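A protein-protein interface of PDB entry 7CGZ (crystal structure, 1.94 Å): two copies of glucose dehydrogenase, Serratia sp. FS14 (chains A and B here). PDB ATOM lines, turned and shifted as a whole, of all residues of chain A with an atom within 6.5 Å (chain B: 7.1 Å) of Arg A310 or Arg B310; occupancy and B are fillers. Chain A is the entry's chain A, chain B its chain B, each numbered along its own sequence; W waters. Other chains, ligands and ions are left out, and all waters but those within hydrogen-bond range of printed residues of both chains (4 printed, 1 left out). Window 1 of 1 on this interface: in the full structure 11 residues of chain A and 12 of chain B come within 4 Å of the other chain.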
ATOM      1  N   HIS A 259     -11.863 -21.377  14.286  1.00  0.00           N
ATOM      2  CA  HIS A 259     -10.550 -21.353  14.899  1.00  0.00           C
ATOM      3  C   HIS A 259     -10.491 -22.507  15.881  1.00  0.00           C
ATOM      4  O   HIS A 259     -11.476 -22.781  16.564  1.00  0.00           O
ATOM      5  CB  HIS A 259     -10.296 -20.022  15.615  1.00  0.00           C
ATOM      6  CG  HIS A 259      -8.847 -19.716  15.819  1.00  0.00           C
ATOM      7  ND1 HIS A 259      -8.236 -19.801  17.051  1.00  0.00           N
ATOM      8  CD2 HIS A 259      -7.887 -19.331  14.945  1.00  0.00           C
ATOM      9  CE1 HIS A 259      -6.960 -19.479  16.929  1.00  0.00           C
ATOM     10  NE2 HIS A 259      -6.723 -19.193  15.660  1.00  0.00           N
ATOM     11  N   TRP A 261      -7.980 -24.886  18.728  1.00  0.00           N
ATOM     12  CA  TRP A 261      -6.816 -25.069  19.596  1.00  0.00           C
ATOM     13  C   TRP A 261      -6.721 -26.547  19.934  1.00  0.00           C
ATOM     14  O   TRP A 261      -7.520 -27.049  20.731  1.00  0.00           O
ATOM     15  CB  TRP A 261      -6.933 -24.283  20.903  1.00  0.00           C
ATOM     16  CG  TRP A 261      -6.928 -22.801  20.854  1.00  0.00           C
ATOM     17  CD1 TRP A 261      -5.876 -21.984  21.138  1.00  0.00           C
ATOM     18  CD2 TRP A 261      -8.049 -21.941  20.595  1.00  0.00           C
ATOM     19  NE1 TRP A 261      -6.256 -20.675  21.039  1.00  0.00           N
ATOM     20  CE2 TRP A 261      -7.588 -20.614  20.714  1.00  0.00           C
ATOM     21  CE3 TRP A 261      -9.393 -22.166  20.262  1.00  0.00           C
ATOM     22  CZ2 TRP A 261      -8.416 -19.509  20.507  1.00  0.00           C
ATOM     23  CZ3 TRP A 261     -10.231 -21.058  20.053  1.00  0.00           C
ATOM     24  CH2 TRP A 261      -9.738 -19.746  20.184  1.00  0.00           C
ATOM     25  N   VAL A 263      -4.543 -28.198  21.745  1.00  0.00           N
ATOM     26  CA  VAL A 263      -4.349 -28.285  23.184  1.00  0.00           C
ATOM     27  C   VAL A 263      -5.239 -27.210  23.795  1.00  0.00           C
ATOM     28  O   VAL A 263      -5.044 -26.022  23.528  1.00  0.00           O
ATOM     29  CB  VAL A 263      -2.875 -28.092  23.573  1.00  0.00           C
ATOM     30  CG1 VAL A 263      -2.706 -28.043  25.092  1.00  0.00           C
ATOM     31  CG2 VAL A 263      -1.991 -29.208  22.960  1.00  0.00           C
ATOM     32  N   PRO A 265      -6.646 -24.382  25.794  1.00  0.00           N
ATOM     33  CA  PRO A 265      -6.338 -23.386  26.831  1.00  0.00           C
ATOM     34  C   PRO A 265      -7.362 -23.367  27.961  1.00  0.00           C
ATOM     35  O   PRO A 265      -7.101 -22.748  28.999  1.00  0.00           O
ATOM     36  CB  PRO A 265      -6.331 -22.057  26.059  1.00  0.00           C
ATOM     37  CG  PRO A 265      -6.228 -22.448  24.597  1.00  0.00           C
ATOM     38  CD  PRO A 265      -6.951 -23.752  24.499  1.00  0.00           C
ATOM     39  N   ALA A 289      -8.903 -17.873  29.475  1.00  0.00           N
ATOM     40  CA  ALA A 289      -8.268 -19.189  29.455  1.00  0.00           C
ATOM     41  C   ALA A 289      -8.128 -19.673  30.892  1.00  0.00           C
ATOM     42  O   ALA A 289      -7.469 -19.021  31.705  1.00  0.00           O
ATOM     43  CB  ALA A 289      -6.909 -19.136  28.747  1.00  0.00           C
ATOM     44  N   GLN A 292      -4.644 -22.341  30.848  1.00  0.00           N
ATOM     45  CA  GLN A 292      -3.426 -21.612  30.513  1.00  0.00           C
ATOM     46  C   GLN A 292      -3.364 -20.241  31.181  1.00  0.00           C
ATOM     47  O   GLN A 292      -2.377 -19.517  30.995  1.00  0.00           O
ATOM     48  CB  GLN A 292      -3.267 -21.517  28.985  1.00  0.00           C
ATOM     49  CG  GLN A 292      -2.979 -22.906  28.365  1.00  0.00           C
ATOM     50  CD  GLN A 292      -2.824 -22.901  26.857  1.00  0.00           C
ATOM     51  OE1 GLN A 292      -2.783 -21.849  26.223  1.00  0.00           O
ATOM     52  NE2 GLN A 292      -2.720 -24.092  26.275  1.00  0.00           N
ATOM     53  N   ALA A 294      -4.708 -17.046  31.298  1.00  0.00           N
ATOM     54  CA  ALA A 294      -4.368 -15.866  30.517  1.00  0.00           C
ATOM     55  C   ALA A 294      -5.637 -15.325  29.879  1.00  0.00           C
ATOM     56  O   ALA A 294      -6.693 -15.955  29.907  1.00  0.00           O
ATOM     57  CB  ALA A 294      -3.295 -16.199  29.460  1.00  0.00           C
ATOM     58  N   LEU A 295      -5.532 -14.128  29.330  1.00  0.00           N
ATOM     59  CA  LEU A 295      -6.617 -13.535  28.563  1.00  0.00           C
ATOM     60  C   LEU A 295      -6.246 -13.618  27.088  1.00  0.00           C
ATOM     61  O   LEU A 295      -5.159 -13.178  26.699  1.00  0.00           O
ATOM     62  CB  LEU A 295      -6.852 -12.079  28.971  1.00  0.00           C
ATOM     63  CG  LEU A 295      -7.856 -11.349  28.071  1.00  0.00           C
ATOM     64  CD1 LEU A 295      -9.240 -11.855  28.360  1.00  0.00           C
ATOM     65  CD2 LEU A 295      -7.769  -9.852  28.331  1.00  0.00           C
ATOM     66  N   ILE A 296      -7.131 -14.182  26.270  1.00  0.00           N
ATOM     67  CA  ILE A 296      -6.838 -14.394  24.854  1.00  0.00           C
ATOM     68  C   ILE A 296      -7.483 -13.272  24.053  1.00  0.00           C
ATOM     69  O   ILE A 296      -8.661 -12.957  24.255  1.00  0.00           O
ATOM     70  CB  ILE A 296      -7.331 -15.773  24.395  1.00  0.00           C
ATOM     71  CG1 ILE A 296      -6.567 -16.865  25.153  1.00  0.00           C
ATOM     72  CG2 ILE A 296      -7.156 -15.940  22.876  1.00  0.00           C
ATOM     73  CD1 ILE A 296      -7.006 -18.273  24.770  1.00  0.00           C
ATOM     74  N   ARG A 297      -6.715 -12.639  23.166  1.00  0.00           N
ATOM     75  CA  ARG A 297      -7.288 -11.612  22.299  1.00  0.00           C
ATOM     76  C   ARG A 297      -7.172 -12.051  20.846  1.00  0.00           C
ATOM     77  O   ARG A 297      -6.063 -12.205  20.331  1.00  0.00           O
ATOM     78  CB  ARG A 297      -6.609 -10.258  22.505  1.00  0.00           C
ATOM     79  CG  ARG A 297      -7.190  -9.187  21.605  1.00  0.00           C
ATOM     80  CD  ARG A 297      -6.587  -7.829  21.883  1.00  0.00           C
ATOM     81  NE  ARG A 297      -5.310  -7.641  21.218  1.00  0.00           N
ATOM     82  CZ  ARG A 297      -5.180  -7.296  19.942  1.00  0.00           C
ATOM     83  NH1 ARG A 297      -6.260  -7.108  19.194  1.00  0.00           N
ATOM     84  NH2 ARG A 297      -3.968  -7.136  19.416  1.00  0.00           N
ATOM     85  N   ALA A 307      -5.256 -13.272  13.975  1.00  0.00           N
ATOM     86  CA  ALA A 307      -4.172 -13.205  14.956  1.00  0.00           C
ATOM     87  C   ALA A 307      -4.707 -13.572  16.332  1.00  0.00           C
ATOM     88  O   ALA A 307      -5.870 -13.301  16.651  1.00  0.00           O
ATOM     89  CB  ALA A 307      -3.542 -11.814  15.003  1.00  0.00           C
ATOM     90  N   GLU A 308      -3.846 -14.184  17.141  1.00  0.00           N
ATOM     91  CA  GLU A 308      -4.147 -14.480  18.536  1.00  0.00           C
ATOM     92  C   GLU A 308      -3.021 -13.926  19.401  1.00  0.00           C
ATOM     93  O   GLU A 308      -1.873 -14.361  19.266  1.00  0.00           O
ATOM     94  CB  GLU A 308      -4.310 -15.990  18.759  1.00  0.00           C
ATOM     95  CG  GLU A 308      -4.236 -16.424  20.236  1.00  0.00           C
ATOM     96  CD  GLU A 308      -4.412 -17.934  20.431  1.00  0.00           C
ATOM     97  OE1 GLU A 308      -4.392 -18.407  21.588  1.00  0.00           O
ATOM     98  OE2 GLU A 308      -4.550 -18.655  19.427  1.00  0.00           O
ATOM     99  N   GLU A 309      -3.346 -12.966  20.272  1.00  0.00           N
ATOM    100  CA  GLU A 309      -2.431 -12.436  21.276  1.00  0.00           C
ATOM    101  C   GLU A 309      -2.764 -12.996  22.657  1.00  0.00           C
ATOM    102  O   GLU A 309      -3.921 -13.286  22.962  1.00  0.00           O
ATOM    103  CB  GLU A 309      -2.490 -10.903  21.321  1.00  0.00           C
ATOM    104  CG  GLU A 309      -1.471 -10.288  22.283  1.00  0.00           C
ATOM    105  CD  GLU A 309      -1.560  -8.768  22.418  1.00  0.00           C
ATOM    106  OE1 GLU A 309      -2.508  -8.159  21.875  1.00  0.00           O
ATOM    107  OE2 GLU A 309      -0.679  -8.180  23.088  1.00  0.00           O
ATOM    108  N   ARG A 310      -1.743 -13.148  23.499  1.00  0.00           N
ATOM    109  CA  ARG A 310      -1.917 -13.598  24.878  1.00  0.00           C
ATOM    110  C   ARG A 310      -1.650 -12.431  25.831  1.00  0.00           C
ATOM    111  O   ARG A 310      -0.630 -11.747  25.705  1.00  0.00           O
ATOM    112  CB  ARG A 310      -0.983 -14.777  25.194  1.00  0.00           C
ATOM    113  CG  ARG A 310      -1.307 -16.060  24.448  1.00  0.00           C
ATOM    114  CD  ARG A 310      -2.756 -16.448  24.671  1.00  0.00           C
ATOM    115  NE  ARG A 310      -3.151 -17.682  24.004  1.00  0.00           N
ATOM    116  CZ  ARG A 310      -2.961 -18.893  24.511  1.00  0.00           C
ATOM    117  NH1 ARG A 310      -2.347 -19.029  25.680  1.00  0.00           N
ATOM    118  NH2 ARG A 310      -3.371 -19.970  23.846  1.00  0.00           N
ATOM    119  N   LEU A 311      -2.565 -12.200  26.784  1.00  0.00           N
ATOM    120  CA  LEU A 311      -2.413 -11.120  27.755  1.00  0.00           C
ATOM    121  C   LEU A 311      -2.590 -11.641  29.174  1.00  0.00           C
ATOM    122  O   LEU A 311      -3.254 -12.657  29.403  1.00  0.00           O
ATOM    123  CB  LEU A 311      -3.438  -9.995  27.516  1.00  0.00           C
ATOM    124  CG  LEU A 311      -3.409  -9.352  26.134  1.00  0.00           C
ATOM    125  CD1 LEU A 311      -4.717  -8.622  25.868  1.00  0.00           C
ATOM    126  CD2 LEU A 311      -2.206  -8.399  26.043  1.00  0.00           C
ATOM    127  N   LEU A 312      -1.982 -10.925  30.126  1.00  0.00           N
ATOM    128  CA  LEU A 312      -2.148 -11.125  31.564  1.00  0.00           C
ATOM    129  C   LEU A 312      -1.568 -12.438  32.062  1.00  0.00           C
ATOM    130  O   LEU A 312      -1.864 -12.847  33.201  1.00  0.00           O
ATOM    131  CB  LEU A 312      -3.624 -11.058  31.990  1.00  0.00           C
ATOM    132  CG  LEU A 312      -4.423  -9.821  31.587  1.00  0.00           C
ATOM    133  CD1 LEU A 312      -5.703  -9.739  32.414  1.00  0.00           C
ATOM    134  CD2 LEU A 312      -3.587  -8.574  31.761  1.00  0.00           C
ATOM    135  N   GLY A 313      -0.740 -13.109  31.257  1.00  0.00           N
ATOM    136  CA  GLY A 313      -0.108 -14.338  31.713  1.00  0.00           C
ATOM    137  C   GLY A 313       0.724 -14.162  32.971  1.00  0.00           C
ATOM    138  O   GLY A 313       0.859 -15.100  33.764  1.00  0.00           O
ATOM    139  N   PRO B   2      -1.425 -17.885   8.819  1.00  0.00           N
ATOM    140  CA  PRO B   2      -0.140 -18.359   8.282  1.00  0.00           C
ATOM    141  C   PRO B   2      -0.270 -19.495   7.263  1.00  0.00           C
ATOM    142  O   PRO B   2      -1.232 -20.268   7.294  1.00  0.00           O
ATOM    143  CB  PRO B   2       0.602 -18.850   9.534  1.00  0.00           C
ATOM    144  CG  PRO B   2      -0.495 -19.168  10.516  1.00  0.00           C
ATOM    145  CD  PRO B   2      -1.535 -18.121  10.268  1.00  0.00           C
ATOM    146  N   TRP B 261       7.166 -17.358  31.563  1.00  0.00           N
ATOM    147  CA  TRP B 261       5.815 -17.910  31.472  1.00  0.00           C
ATOM    148  C   TRP B 261       5.509 -18.682  32.750  1.00  0.00           C
ATOM    149  O   TRP B 261       6.180 -19.672  33.052  1.00  0.00           O
ATOM    150  CB  TRP B 261       5.682 -18.857  30.277  1.00  0.00           C
ATOM    151  CG  TRP B 261       5.754 -18.255  28.910  1.00  0.00           C
ATOM    152  CD1 TRP B 261       4.713 -18.083  28.042  1.00  0.00           C
ATOM    153  CD2 TRP B 261       6.928 -17.811  28.216  1.00  0.00           C
ATOM    154  NE1 TRP B 261       5.162 -17.542  26.863  1.00  0.00           N
ATOM    155  CE2 TRP B 261       6.515 -17.365  26.941  1.00  0.00           C
ATOM    156  CE3 TRP B 261       8.284 -17.752  28.544  1.00  0.00           C
ATOM    157  CZ2 TRP B 261       7.408 -16.853  25.999  1.00  0.00           C
ATOM    158  CZ3 TRP B 261       9.172 -17.230  27.607  1.00  0.00           C
ATOM    159  CH2 TRP B 261       8.724 -16.793  26.349  1.00  0.00           C
ATOM    160  N   VAL B 263       2.774 -20.489  33.193  1.00  0.00           N
ATOM    161  CA  VAL B 263       2.339 -21.765  32.638  1.00  0.00           C
ATOM    162  C   VAL B 263       3.290 -22.102  31.498  1.00  0.00           C
ATOM    163  O   VAL B 263       3.376 -21.359  30.512  1.00  0.00           O
ATOM    164  CB  VAL B 263       0.881 -21.704  32.155  1.00  0.00           C
ATOM    165  CG1 VAL B 263       0.462 -23.036  31.552  1.00  0.00           C
ATOM    166  CG2 VAL B 263      -0.057 -21.309  33.298  1.00  0.00           C
ATOM    167  N   SER B 264       4.001 -23.221  31.623  1.00  0.00           N
ATOM    168  CA  SER B 264       5.113 -23.510  30.720  1.00  0.00           C
ATOM    169  C   SER B 264       4.594 -24.011  29.379  1.00  0.00           C
ATOM    170  O   SER B 264       3.928 -25.050  29.333  1.00  0.00           O
ATOM    171  CB  SER B 264       6.060 -24.547  31.321  1.00  0.00           C
ATOM    172  OG  SER B 264       7.042 -23.927  32.133  1.00  0.00           O
ATOM    173  N   PRO B 265       4.883 -23.324  28.275  1.00  0.00           N
ATOM    174  CA  PRO B 265       4.535 -23.880  26.963  1.00  0.00           C
ATOM    175  C   PRO B 265       5.447 -25.018  26.535  1.00  0.00           C
ATOM    176  O   PRO B 265       5.093 -25.747  25.601  1.00  0.00           O
ATOM    177  CB  PRO B 265       4.664 -22.675  26.020  1.00  0.00           C
ATOM    178  CG  PRO B 265       4.746 -21.446  26.927  1.00  0.00           C
ATOM    179  CD  PRO B 265       5.433 -21.962  28.168  1.00  0.00           C
ATOM    180  N   ALA B 289       6.689 -24.395  20.952  1.00  0.00           N
ATOM    181  CA  ALA B 289       6.096 -24.915  22.182  1.00  0.00           C
ATOM    182  C   ALA B 289       5.844 -26.406  22.017  1.00  0.00           C
ATOM    183  O   ALA B 289       5.054 -26.815  21.157  1.00  0.00           O
ATOM    184  CB  ALA B 289       4.790 -24.190  22.528  1.00  0.00           C
ATOM    185  N   GLN B 292       2.381 -27.203  24.581  1.00  0.00           N
ATOM    186  CA  GLN B 292       1.164 -26.565  24.093  1.00  0.00           C
ATOM    187  C   GLN B 292       1.000 -26.667  22.579  1.00  0.00           C
ATOM    188  O   GLN B 292      -0.005 -26.173  22.050  1.00  0.00           O
ATOM    189  CB  GLN B 292       1.122 -25.098  24.536  1.00  0.00           C
ATOM    190  CG  GLN B 292       0.834 -24.910  26.030  1.00  0.00           C
ATOM    191  CD  GLN B 292       0.963 -23.462  26.491  1.00  0.00           C
ATOM    192  OE1 GLN B 292       1.079 -22.547  25.673  1.00  0.00           O
ATOM    193  NE2 GLN B 292       0.951 -23.250  27.808  1.00  0.00           N
ATOM    194  N   LYS B 293       1.957 -27.294  21.882  1.00  0.00           N
ATOM    195  CA  LYS B 293       1.865 -27.634  20.455  1.00  0.00           C
ATOM    196  C   LYS B 293       1.467 -26.434  19.594  1.00  0.00           C
ATOM    197  O   LYS B 293       0.437 -26.431  18.917  1.00  0.00           O
ATOM    198  CB  LYS B 293       0.907 -28.809  20.223  1.00  0.00           C
ATOM    199  CG  LYS B 293       1.176 -29.984  21.146  1.00  0.00           C
ATOM    200  CD  LYS B 293       0.343 -31.224  20.819  1.00  0.00           C
ATOM    201  CE  LYS B 293       0.931 -32.412  21.566  1.00  0.00           C
ATOM    202  NZ  LYS B 293      -0.036 -33.480  21.898  1.00  0.00           N
ATOM    203  N   ALA B 294       2.335 -25.426  19.590  1.00  0.00           N
ATOM    204  CA  ALA B 294       2.069 -24.188  18.868  1.00  0.00           C
ATOM    205  C   ALA B 294       3.390 -23.477  18.615  1.00  0.00           C
ATOM    206  O   ALA B 294       4.443 -23.885  19.112  1.00  0.00           O
ATOM    207  CB  ALA B 294       1.106 -23.282  19.648  1.00  0.00           C
ATOM    208  N   LEU B 295       3.318 -22.404  17.831  1.00  0.00           N
ATOM    209  CA  LEU B 295       4.458 -21.540  17.559  1.00  0.00           C
ATOM    210  C   LEU B 295       4.234 -20.209  18.256  1.00  0.00           C
ATOM    211  O   LEU B 295       3.202 -19.558  18.046  1.00  0.00           O
ATOM    212  CB  LEU B 295       4.648 -21.334  16.058  1.00  0.00           C
ATOM    213  CG  LEU B 295       5.873 -20.502  15.673  1.00  0.00           C
ATOM    214  CD1 LEU B 295       7.183 -21.239  16.017  1.00  0.00           C
ATOM    215  CD2 LEU B 295       5.796 -20.146  14.187  1.00  0.00           C
ATOM    216  N   ILE B 296       5.166 -19.826  19.102  1.00  0.00           N
ATOM    217  CA  ILE B 296       5.063 -18.571  19.832  1.00  0.00           C
ATOM    218  C   ILE B 296       5.808 -17.503  19.047  1.00  0.00           C
ATOM    219  O   ILE B 296       6.921 -17.737  18.548  1.00  0.00           O
ATOM    220  CB  ILE B 296       5.630 -18.717  21.259  1.00  0.00           C
ATOM    221  CG1 ILE B 296       4.844 -19.766  22.054  1.00  0.00           C
ATOM    222  CG2 ILE B 296       5.643 -17.365  21.983  1.00  0.00           C
ATOM    223  CD1 ILE B 296       5.510 -20.124  23.389  1.00  0.00           C
ATOM    224  N   ARG B 297       5.201 -16.326  18.937  1.00  0.00           N
ATOM    225  CA  ARG B 297       5.830 -15.180  18.294  1.00  0.00           C
ATOM    226  C   ARG B 297       5.876 -14.007  19.267  1.00  0.00           C
ATOM    227  O   ARG B 297       4.828 -13.501  19.688  1.00  0.00           O
ATOM    228  CB  ARG B 297       5.075 -14.814  17.020  1.00  0.00           C
ATOM    229  CG  ARG B 297       5.589 -13.587  16.331  1.00  0.00           C
ATOM    230  CD  ARG B 297       4.562 -13.121  15.304  1.00  0.00           C
ATOM    231  NE  ARG B 297       4.942 -11.829  14.757  1.00  0.00           N
ATOM    232  CZ  ARG B 297       4.105 -10.824  14.557  1.00  0.00           C
ATOM    233  NH1 ARG B 297       2.813 -10.959  14.840  1.00  0.00           N
ATOM    234  NH2 ARG B 297       4.568  -9.689  14.054  1.00  0.00           N
ATOM    235  N   ALA B 307       4.723  -8.008  23.052  1.00  0.00           N
ATOM    236  CA  ALA B 307       3.506  -8.759  22.758  1.00  0.00           C
ATOM    237  C   ALA B 307       3.861 -10.222  22.542  1.00  0.00           C
ATOM    238  O   ALA B 307       4.954 -10.550  22.054  1.00  0.00           O
ATOM    239  CB  ALA B 307       2.778  -8.215  21.527  1.00  0.00           C
ATOM    240  N   GLU B 308       2.921 -11.092  22.907  1.00  0.00           N
ATOM    241  CA  GLU B 308       3.042 -12.525  22.687  1.00  0.00           C
ATOM    242  C   GLU B 308       1.877 -12.998  21.834  1.00  0.00           C
ATOM    243  O   GLU B 308       0.710 -12.758  22.174  1.00  0.00           O
ATOM    244  CB  GLU B 308       3.072 -13.318  23.994  1.00  0.00           C
ATOM    245  CG  GLU B 308       2.913 -14.817  23.709  1.00  0.00           C
ATOM    246  CD  GLU B 308       3.024 -15.695  24.934  1.00  0.00           C
ATOM    247  OE1 GLU B 308       3.173 -15.156  26.044  1.00  0.00           O
ATOM    248  OE2 GLU B 308       2.946 -16.935  24.784  1.00  0.00           O
ATOM    249  N   GLU B 309       2.191 -13.662  20.726  1.00  0.00           N
ATOM    250  CA  GLU B 309       1.175 -14.187  19.826  1.00  0.00           C
ATOM    251  C   GLU B 309       1.393 -15.676  19.601  1.00  0.00           C
ATOM    252  O   GLU B 309       2.491 -16.194  19.809  1.00  0.00           O
ATOM    253  CB  GLU B 309       1.179 -13.419  18.509  1.00  0.00           C
ATOM    254  CG  GLU B 309       0.841 -11.951  18.746  1.00  0.00           C
ATOM    255  CD  GLU B 309       0.632 -11.181  17.466  1.00  0.00           C
ATOM    256  OE1 GLU B 309       0.997 -11.713  16.388  1.00  0.00           O
ATOM    257  OE2 GLU B 309       0.108 -10.046  17.545  1.00  0.00           O
ATOM    258  N   ARG B 310       0.321 -16.373  19.216  1.00  0.00           N
ATOM    259  CA  ARG B 310       0.345 -17.813  18.990  1.00  0.00           C
ATOM    260  C   ARG B 310       0.007 -18.113  17.535  1.00  0.00           C
ATOM    261  O   ARG B 310      -0.905 -17.505  16.957  1.00  0.00           O
ATOM    262  CB  ARG B 310      -0.648 -18.578  19.899  1.00  0.00           C
ATOM    263  CG  ARG B 310      -0.369 -18.507  21.391  1.00  0.00           C
ATOM    264  CD  ARG B 310       1.076 -18.862  21.693  1.00  0.00           C
ATOM    265  NE  ARG B 310       1.394 -18.792  23.120  1.00  0.00           N
ATOM    266  CZ  ARG B 310       1.105 -19.741  24.009  1.00  0.00           C
ATOM    267  NH1 ARG B 310       0.473 -20.842  23.630  1.00  0.00           N
ATOM    268  NH2 ARG B 310       1.476 -19.593  25.276  1.00  0.00           N
ATOM    269  N   LEU B 311       0.736 -19.069  16.958  1.00  0.00           N
ATOM    270  CA  LEU B 311       0.512 -19.544  15.600  1.00  0.00           C
ATOM    271  C   LEU B 311       0.439 -21.063  15.610  1.00  0.00           C
ATOM    272  O   LEU B 311       1.010 -21.718  16.487  1.00  0.00           O
ATOM    273  CB  LEU B 311       1.637 -19.095  14.640  1.00  0.00           C
ATOM    274  CG  LEU B 311       1.789 -17.608  14.291  1.00  0.00           C
ATOM    275  CD1 LEU B 311       2.357 -16.797  15.442  1.00  0.00           C
ATOM    276  CD2 LEU B 311       2.683 -17.462  13.081  1.00  0.00           C
ATOM    277  N   LEU B 312      -0.281 -21.619  14.632  1.00  0.00           N
ATOM    278  CA  LEU B 312      -0.270 -23.054  14.327  1.00  0.00           C
ATOM    279  C   LEU B 312      -0.815 -23.923  15.459  1.00  0.00           C
ATOM    280  O   LEU B 312      -0.602 -25.141  15.462  1.00  0.00           O
ATOM    281  CB  LEU B 312       1.143 -23.535  13.946  1.00  0.00           C
ATOM    282  CG  LEU B 312       1.947 -22.697  12.953  1.00  0.00           C
ATOM    283  CD1 LEU B 312       3.286 -23.380  12.643  1.00  0.00           C
ATOM    284  CD2 LEU B 312       1.179 -22.473  11.683  1.00  0.00           C
ATOM    285  N   GLY B 313      -1.549 -23.347  16.415  1.00  0.00           N
ATOM    286  CA  GLY B 313      -2.094 -24.148  17.503  1.00  0.00           C
ATOM    287  C   GLY B 313      -3.193 -25.111  17.089  1.00  0.00           C
ATOM    288  O   GLY B 313      -3.563 -25.988  17.877  1.00  0.00           O
HETATM  289  O   HOH W   1      -2.388 -24.053  22.916  1.00  0.00           O
HETATM  290  O   HOH W   2      -1.503 -21.893  21.901  1.00  0.00           O
HETATM  291  O   HOH W   3       0.857  -9.823  24.433  1.00  0.00           O
HETATM  292  O   HOH W   4      -1.535 -15.426  15.874  1.00  0.00           O
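The backbone carbonyl oxygen of Glu A308 is in hydrogen-bond range of the backbone NH of Arg B310.
The backbone carbonyl oxygen (O) of Glu B308 sits at hydrogen-bond distance from the backbone NH (N) of Arg A310 (2.8 Å).
The side-chain carboxylate (OE1) of Glu A308 sits at hydrogen-bond distance from the indole nitrogen (NE1) of Trp A261.
O of Pro A265 sits at hydrogen-bond distance from N of Gln A292 (3.1 Å).
OE2 of Glu B308 lies within hydrogen-bond range of NE1 of Trp B261, 3.1 Å away.
The backbone NH (N) of Gln B292 lies within hydrogen-bond range of the backbone carbonyl oxygen (O) of Pro B265.
The guanidinium group (NH1) of Arg B297 lies within salt-bridge range of the side-chain carboxylate (OE1) of Glu B309 (2.5 Å).
OE2 of Glu B308 lies within salt-bridge range of NE of Arg B310 (2.9 Å).
Among the printed residues, pairs that only touch across the chains: Trp A261 with Gly B313, Val A263 with Gln B292, Val A263 with Lys B293, Gln A292 with Val B263, Gln A292 with Gln B292, Glu A308 with Glu B309, Glu A309 with Ala B307, Glu A309 with Glu B308 and Arg A310 with Arg B310.
Arg A310 touches just these residues of chain B: Glu B308 (2.8 Å) and Arg B310 (3.9 Å).
Of the printed residues of chain B, Glu A308 touches Glu B309 and Arg B310.
Of the printed residues of chain A, Glu B308 touches Glu A309 (3.3 Å) and Arg A310 (2.8 Å).
Of the printed residues of chain A, Gln B292 touches Val A263 and Gln A292.
Leu A312 touches none of the printed residues of chain B.
Ala A294 touches none of the printed residues of chain B.
The nearest residue of chain B that does not touch Arg A310 is Glu B309 (4.8 Å).
The nearest residue of chain A that does not touch Arg B310 is Gln A292 (4.3 Å).
The nearest printed residue of chain A that does not touch Glu B309 is Glu A309 (4.2 Å).
Hydrophobic or aromatic side chains of chain B that line the printed part of chain A: Val B263 and Ala B307.
Hydrophobic or aromatic side chains of chain A within 4 Å of the printed part of chain B: Val A263.
Among the printed residues, 11 pairs touch across the chains.
Trp A261 touches Gly B313, but with the chains exchanged Gly A313 does not touch Trp B261 (6.0 Å).
Val A263 touches Gln B292, and with the chains exchanged Gln A292 touches Val B263.
Gln A292 touches its own counterpart, Gln B292.
Glu A309 touches Ala B307, but with the chains exchanged Ala A307 does not touch Glu B309 (4.7 Å).
Of the 11 pairs that touch across the chains among the printed residues, 8 have their exchanged pair printed and touching as well.
Water W4 bridges the backbone carbonyl oxygen of Arg B310 (2.4 Å) and the backbone NH of Glu A308 (2.9 Å).
Water W3 lies within hydrogen-bond range of the side-chain carboxylate of Glu A309 (2.6 Å), the backbone carbonyl oxygen of Arg A310 (2.7 Å) and the backbone NH of Glu B308 (2.9 Å).
Water W2 lies within hydrogen-bond range of NH1 of Arg B310 (2.8 Å) and NH2 of Arg A310 (3.3 Å).
Water W1 lies within hydrogen-bond range of O of Gln B292, O of Val A263 and NE2 of Gln A292.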
